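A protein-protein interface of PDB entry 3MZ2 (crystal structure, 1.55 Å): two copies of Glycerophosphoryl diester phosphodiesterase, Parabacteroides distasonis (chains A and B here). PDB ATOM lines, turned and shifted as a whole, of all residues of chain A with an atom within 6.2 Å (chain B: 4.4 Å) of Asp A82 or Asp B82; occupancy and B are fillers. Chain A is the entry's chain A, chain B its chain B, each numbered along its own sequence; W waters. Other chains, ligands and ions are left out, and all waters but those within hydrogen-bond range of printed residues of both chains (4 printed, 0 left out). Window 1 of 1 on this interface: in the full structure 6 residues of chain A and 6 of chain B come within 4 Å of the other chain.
His A80 touches Asp B82, but with the chains exchanged Asp A82 does not touch His B80 (4.3 Å).
Asp A81 touches Asp B82, and with the chains exchanged Asp A82 touches Asp B81.
Asp A81 touches Thr B83, and with the chains exchanged Thr A83 touches Asp B81.
Thr A83 touches its own counterpart, Thr B83.
The side-chain carboxylate (OD2) of Asp A82 sits at hydrogen-bond distance from the backbone NH (N) of Asp B82 (2.8 Å).
OG1 of Thr B83 lies within hydrogen-bond range of OG1 of Thr A83 (2.4 Å).
Printed residues of chain B that touch a printed residue of chain A: Asp B81, Asp B82 and Thr B83.
Along chain B the printed residues that touch a printed residue of chain A span positions 81 to 83.
Hydrophobic or aromatic side chains of chain A that line the printed part of chain B: His A80.
Among the printed residues, 7 pairs touch across the chains.
Among the printed residues, pairs that only touch across the chains: His A80 with Asp B82, Asp A81 with Thr B83, Asp A82 with Asp B81, Asp A81 with Asp B82 and Thr A83 with Asp B81.
The backbone carbonyl oxygen of His A80 is in hydrogen-bond range of the guanidinium group of Arg A69 (2.9 Å).
The guanidinium group (NE) of Arg A69 sits at hydrogen-bond distance from the backbone carbonyl oxygen (O) of Asp A81, at 3.3 Å.
OD1 of Asp A82 lies within salt-bridge range of NH2 of Arg A69, 3.1 Å away.
OD1 of Asp A81 lies within hydrogen-bond range of ND1 of His A80.
A ring nitrogen (ND1) of His B80 sits at hydrogen-bond distance from the side-chain carboxylate of Asp B81, 2.7 Å away.
The backbone carbonyl oxygen (O) of Asp B82 lies within hydrogen-bond range of the backbone NH (N) of Val B94, at 3.3 Å.
Of chain B, only Asp B81 and Asp B82 come within 4 Å of Asp A82.
Printed residues of chain A within 4 Å of Asp B82: His A80 (3.3 Å), Asp A81 (3.5 Å) and Asp A82 (2.8 Å).
Printed residues of chain A within 4 Å of Asp B81: Asp A82 and Thr A83.
Printed residues of chain B within 4 Å of Asp A81: Asp B82 and Thr B83.
Printed residues of chain B within 4 Å of His A80: Asp B82.
The nearest printed residue of chain B that does not touch Asp A81 is Lys B93 (5.6 Å).
Water W4 lies within hydrogen-bond range of OD2 of Asp A82 (2.6 Å) and O of His B80 (3.0 Å).
Water W2 lies within hydrogen-bond range of OD2 of Asp B81 (2.7 Å) and O of Asp A82 (2.9 Å).
Water W1 lies within hydrogen-bond range of the side-chain carboxylate (OD1) of Asp A81 and the side-chain carboxylate (OD2) of Asp B82.
Water W3 lies within hydrogen-bond range of the side-chain carboxylate (OD2) of Asp B82 (2.9 Å) and the backbone carbonyl oxygen (O) of His A80 (3.2 Å).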
ATOM      1  N   ARG A  69     -19.699  -2.715 -22.882  1.00  0.00           N
ATOM      2  CA  ARG A  69     -19.265  -2.443 -21.530  1.00  0.00           C
ATOM      3  C   ARG A  69     -19.517  -0.970 -21.183  1.00  0.00           C
ATOM      4  O   ARG A  69     -19.829  -0.141 -22.029  1.00  0.00           O
ATOM      5  CB  ARG A  69     -17.781  -2.796 -21.303  1.00  0.00           C
ATOM      6  CG  ARG A  69     -16.817  -1.970 -22.075  1.00  0.00           C
ATOM      7  CD  ARG A  69     -15.366  -2.091 -21.572  1.00  0.00           C
ATOM      8  NE  ARG A  69     -14.832  -3.473 -21.506  1.00  0.00           N
ATOM      9  CZ  ARG A  69     -14.615  -4.136 -20.379  1.00  0.00           C
ATOM     10  NH1 ARG A  69     -14.947  -3.619 -19.207  1.00  0.00           N
ATOM     11  NH2 ARG A  69     -14.119  -5.363 -20.448  1.00  0.00           N
ATOM     12  N   PHE A  79     -15.997  -2.301 -26.511  1.00  0.00           N
ATOM     13  CA  PHE A  79     -14.588  -2.335 -26.202  1.00  0.00           C
ATOM     14  C   PHE A  79     -14.317  -3.621 -25.405  1.00  0.00           C
ATOM     15  O   PHE A  79     -14.935  -3.834 -24.355  1.00  0.00           O
ATOM     16  CB  PHE A  79     -14.183  -1.102 -25.355  1.00  0.00           C
ATOM     17  CG  PHE A  79     -12.714  -0.852 -25.357  1.00  0.00           C
ATOM     18  CD1 PHE A  79     -12.133  -0.117 -26.387  1.00  0.00           C
ATOM     19  CD2 PHE A  79     -11.902  -1.379 -24.367  1.00  0.00           C
ATOM     20  CE1 PHE A  79     -10.787   0.086 -26.422  1.00  0.00           C
ATOM     21  CE2 PHE A  79     -10.545  -1.180 -24.419  1.00  0.00           C
ATOM     22  CZ  PHE A  79      -9.999  -0.434 -25.436  1.00  0.00           C
ATOM     23  N   HIS A  80     -13.392  -4.453 -25.869  1.00  0.00           N
ATOM     24  CA  HIS A  80     -13.226  -5.773 -25.253  1.00  0.00           C
ATOM     25  C   HIS A  80     -12.538  -5.780 -23.879  1.00  0.00           C
ATOM     26  O   HIS A  80     -13.055  -6.344 -22.931  1.00  0.00           O
ATOM     27  CB  HIS A  80     -12.488  -6.729 -26.193  1.00  0.00           C
ATOM     28  CG  HIS A  80     -12.260  -8.082 -25.588  1.00  0.00           C
ATOM     29  ND1 HIS A  80     -11.148  -8.359 -24.813  1.00  0.00           N
ATOM     30  CD2 HIS A  80     -13.043  -9.184 -25.531  1.00  0.00           C
ATOM     31  CE1 HIS A  80     -11.234  -9.604 -24.370  1.00  0.00           C
ATOM     32  NE2 HIS A  80     -12.359 -10.133 -24.809  1.00  0.00           N
ATOM     33  N   ASP A  81     -11.359  -5.185 -23.820  1.00  0.00           N
ATOM     34  CA  ASP A  81     -10.450  -5.344 -22.663  1.00  0.00           C
ATOM     35  C   ASP A  81     -10.838  -4.502 -21.462  1.00  0.00           C
ATOM     36  O   ASP A  81     -11.527  -3.478 -21.585  1.00  0.00           O
ATOM     37  CB  ASP A  81      -9.014  -4.968 -23.020  1.00  0.00           C
ATOM     38  CG  ASP A  81      -8.383  -5.875 -24.045  1.00  0.00           C
ATOM     39  OD1 ASP A  81      -8.915  -6.976 -24.351  1.00  0.00           O
ATOM     40  OD2 ASP A  81      -7.332  -5.471 -24.583  1.00  0.00           O
ATOM     41  N   ASP A  82     -10.294  -4.937 -20.320  1.00  0.00           N
ATOM     42  CA  ASP A  82     -10.424  -4.250 -19.048  1.00  0.00           C
ATOM     43  C   ASP A  82      -9.515  -3.023 -19.000  1.00  0.00           C
ATOM     44  O   ASP A  82      -9.630  -2.215 -18.118  1.00  0.00           O
ATOM     45  CB  ASP A  82     -10.066  -5.205 -17.859  1.00  0.00           C
ATOM     46  CG  ASP A  82     -11.036  -6.369 -17.732  1.00  0.00           C
ATOM     47  OD1 ASP A  82     -12.232  -6.236 -18.138  1.00  0.00           O
ATOM     48  OD2 ASP A  82     -10.605  -7.435 -17.262  1.00  0.00           O
ATOM     49  N   THR A  83      -8.558  -2.926 -19.900  1.00  0.00           N
ATOM     50  CA  THR A  83      -7.699  -1.732 -19.948  1.00  0.00           C
ATOM     51  C   THR A  83      -7.695  -1.207 -21.384  1.00  0.00           C
ATOM     52  O   THR A  83      -7.903  -1.970 -22.335  1.00  0.00           O
ATOM     53  CB  THR A  83      -6.268  -2.049 -19.458  1.00  0.00           C
ATOM     54  OG1 THR A  83      -5.617  -2.959 -20.362  1.00  0.00           O
ATOM     55  CG2 THR A  83      -6.317  -2.669 -18.101  1.00  0.00           C
ATOM     56  N   LEU A  84      -7.458   0.088 -21.532  1.00  0.00           N
ATOM     57  CA  LEU A  84      -7.466   0.753 -22.853  1.00  0.00           C
ATOM     58  C   LEU A  84      -6.256   0.536 -23.763  1.00  0.00           C
ATOM     59  O   LEU A  84      -6.404   0.730 -24.945  1.00  0.00           O
ATOM     60  CB  LEU A  84      -7.687   2.262 -22.663  1.00  0.00           C
ATOM     61  CG  LEU A  84      -9.054   2.674 -22.125  1.00  0.00           C
ATOM     62  CD1 LEU A  84      -9.040   4.119 -21.524  1.00  0.00           C
ATOM     63  CD2 LEU A  84     -10.046   2.521 -23.260  1.00  0.00           C
ATOM     64  N   GLY A  92      -5.663   3.170 -18.599  1.00  0.00           N
ATOM     65  CA  GLY A  92      -6.667   3.004 -17.541  1.00  0.00           C
ATOM     66  C   GLY A  92      -7.819   2.139 -18.025  1.00  0.00           C
ATOM     67  O   GLY A  92      -7.713   1.518 -19.084  1.00  0.00           O
ATOM     68  N   LYS A  93      -8.901   2.119 -17.234  1.00  0.00           N
ATOM     69  CA  LYS A  93     -10.120   1.334 -17.489  1.00  0.00           C
ATOM     70  C   LYS A  93     -11.101   2.172 -18.317  1.00  0.00           C
ATOM     71  O   LYS A  93     -11.229   3.381 -18.078  1.00  0.00           O
ATOM     72  CB  LYS A  93     -10.839   1.044 -16.143  1.00  0.00           C
ATOM     73  CG  LYS A  93     -10.103   0.155 -15.151  1.00  0.00           C
ATOM     74  CD  LYS A  93     -10.968  -0.283 -13.964  1.00  0.00           C
ATOM     75  CE  LYS A  93     -11.528   0.897 -13.174  1.00  0.00           C
ATOM     76  NZ  LYS A  93     -12.378   0.460 -12.020  1.00  0.00           N
ATOM     77  N   VAL A  94     -11.856   1.553 -19.201  1.00  0.00           N
ATOM     78  CA  VAL A  94     -12.987   2.247 -19.838  1.00  0.00           C
ATOM     79  C   VAL A  94     -13.885   2.894 -18.757  1.00  0.00           C
ATOM     80  O   VAL A  94     -14.342   4.033 -18.921  1.00  0.00           O
ATOM     81  CB  VAL A  94     -13.828   1.296 -20.740  1.00  0.00           C
ATOM     82  CG1 VAL A  94     -15.183   1.871 -21.078  1.00  0.00           C
ATOM     83  CG2 VAL A  94     -13.090   0.945 -22.032  1.00  0.00           C
ATOM     84  N   LYS A 140     -19.792  -8.405 -20.716  1.00  0.00           N
ATOM     85  CA  LYS A 140     -18.714  -7.880 -19.897  1.00  0.00           C
ATOM     86  C   LYS A 140     -19.341  -7.406 -18.583  1.00  0.00           C
ATOM     87  O   LYS A 140     -19.663  -8.225 -17.728  1.00  0.00           O
ATOM     88  CB  LYS A 140     -17.958  -6.752 -20.630  1.00  0.00           C
ATOM     89  CG  LYS A 140     -17.389  -7.141 -22.006  1.00  0.00           C
ATOM     90  CD  LYS A 140     -16.113  -7.959 -21.899  1.00  0.00           C
ATOM     91  CE  LYS A 140     -15.741  -8.547 -23.235  1.00  0.00           C
ATOM     92  NZ  LYS A 140     -16.815  -9.447 -23.725  1.00  0.00           N
ATOM     93  N   ARG B  69      -6.850 -17.043 -13.125  1.00  0.00           N
ATOM     94  CA  ARG B  69      -6.934 -17.034 -14.564  1.00  0.00           C
ATOM     95  C   ARG B  69      -5.773 -17.806 -15.178  1.00  0.00           C
ATOM     96  O   ARG B  69      -4.779 -18.133 -14.512  1.00  0.00           O
ATOM     97  CB  ARG B  69      -7.018 -15.588 -15.144  1.00  0.00           C
ATOM     98  CG  ARG B  69      -5.813 -14.730 -14.914  1.00  0.00           C
ATOM     99  CD  ARG B  69      -5.910 -13.396 -15.686  1.00  0.00           C
ATOM    100  NE  ARG B  69      -7.184 -12.702 -15.500  1.00  0.00           N
ATOM    101  CZ  ARG B  69      -8.189 -12.654 -16.382  1.00  0.00           C
ATOM    102  NH1 ARG B  69      -8.154 -13.353 -17.517  1.00  0.00           N
ATOM    103  NH2 ARG B  69      -9.267 -11.929 -16.120  1.00  0.00           N
ATOM    104  N   HIS B  80      -6.485  -9.962 -11.681  1.00  0.00           N
ATOM    105  CA  HIS B  80      -7.883  -9.610 -11.959  1.00  0.00           C
ATOM    106  C   HIS B  80      -8.152  -9.333 -13.445  1.00  0.00           C
ATOM    107  O   HIS B  80      -9.046  -9.930 -14.079  1.00  0.00           O
ATOM    108  CB  HIS B  80      -8.345  -8.425 -11.097  1.00  0.00           C
ATOM    109  CG  HIS B  80      -9.749  -8.017 -11.394  1.00  0.00           C
ATOM    110  ND1 HIS B  80     -10.050  -7.082 -12.359  1.00  0.00           N
ATOM    111  CD2 HIS B  80     -10.929  -8.498 -10.949  1.00  0.00           C
ATOM    112  CE1 HIS B  80     -11.366  -6.985 -12.478  1.00  0.00           C
ATOM    113  NE2 HIS B  80     -11.926  -7.833 -11.634  1.00  0.00           N
ATOM    114  N   ASP B  81      -7.406  -8.418 -14.022  1.00  0.00           N
ATOM    115  CA  ASP B  81      -7.808  -7.903 -15.332  1.00  0.00           C
ATOM    116  C   ASP B  81      -7.452  -8.895 -16.427  1.00  0.00           C
ATOM    117  O   ASP B  81      -6.490  -9.634 -16.316  1.00  0.00           O
ATOM    118  CB  ASP B  81      -7.102  -6.599 -15.629  1.00  0.00           C
ATOM    119  CG  ASP B  81      -7.597  -5.450 -14.822  1.00  0.00           C
ATOM    120  OD1 ASP B  81      -8.604  -5.545 -14.121  1.00  0.00           O
ATOM    121  OD2 ASP B  81      -6.911  -4.397 -14.857  1.00  0.00           O
ATOM    122  N   ASP B  82      -8.154  -8.832 -17.551  1.00  0.00           N
ATOM    123  CA  ASP B  82      -7.740  -9.707 -18.637  1.00  0.00           C
ATOM    124  C   ASP B  82      -6.378  -9.241 -19.278  1.00  0.00           C
ATOM    125  O   ASP B  82      -5.587 -10.086 -19.777  1.00  0.00           O
ATOM    126  CB  ASP B  82      -8.881  -9.931 -19.638  1.00  0.00           C
ATOM    127  CG  ASP B  82      -9.230  -8.722 -20.423  1.00  0.00           C
ATOM    128  OD1 ASP B  82      -9.051  -7.566 -19.987  1.00  0.00           O
ATOM    129  OD2 ASP B  82      -9.721  -8.959 -21.549  1.00  0.00           O
ATOM    130  N   THR B  83      -6.058  -7.951 -19.153  1.00  0.00           N
ATOM    131  CA  THR B  83      -4.800  -7.400 -19.661  1.00  0.00           C
ATOM    132  C   THR B  83      -3.933  -6.900 -18.489  1.00  0.00           C
ATOM    133  O   THR B  83      -4.428  -6.721 -17.378  1.00  0.00           O
ATOM    134  CB  THR B  83      -5.075  -6.303 -20.648  1.00  0.00           C
ATOM    135  OG1 THR B  83      -5.944  -5.349 -20.038  1.00  0.00           O
ATOM    136  CG2 THR B  83      -5.755  -6.925 -21.922  1.00  0.00           C
ATOM    137  N   LYS B  93      -2.218  -9.533 -22.776  1.00  0.00           N
ATOM    138  CA  LYS B  93      -3.079 -10.405 -22.003  1.00  0.00           C
ATOM    139  C   LYS B  93      -2.224 -11.342 -21.175  1.00  0.00           C
ATOM    140  O   LYS B  93      -1.186 -11.814 -21.661  1.00  0.00           O
ATOM    141  CB  LYS B  93      -3.859 -11.351 -22.945  1.00  0.00           C
ATOM    142  CG  LYS B  93      -4.921 -10.809 -23.887  1.00  0.00           C
ATOM    143  CD  LYS B  93      -5.731 -12.005 -24.494  1.00  0.00           C
ATOM    144  CE  LYS B  93      -4.888 -12.845 -25.425  1.00  0.00           C
ATOM    145  NZ  LYS B  93      -5.172 -14.316 -25.540  1.00  0.00           N
ATOM    146  N   VAL B  94      -2.686 -11.682 -19.978  1.00  0.00           N
ATOM    147  CA  VAL B  94      -2.088 -12.738 -19.185  1.00  0.00           C
ATOM    148  C   VAL B  94      -1.967 -14.032 -20.015  1.00  0.00           C
ATOM    149  O   VAL B  94      -0.931 -14.717 -19.979  1.00  0.00           O
ATOM    150  CB  VAL B  94      -2.940 -13.025 -17.920  1.00  0.00           C
ATOM    151  CG1 VAL B  94      -2.416 -14.263 -17.164  1.00  0.00           C
ATOM    152  CG2 VAL B  94      -3.056 -11.701 -17.030  1.00  0.00           C
HETATM  153  O   HOH W   1      -7.559  -9.292 -23.947  1.00  0.00           O
HETATM  154  O   HOH W   2      -8.211  -2.183 -15.619  1.00  0.00           O
HETATM  155  O   HOH W   3     -12.573  -9.039 -21.315  1.00  0.00           O
HETATM  156  O   HOH W   4     -11.546  -8.957 -15.415  1.00  0.00           O
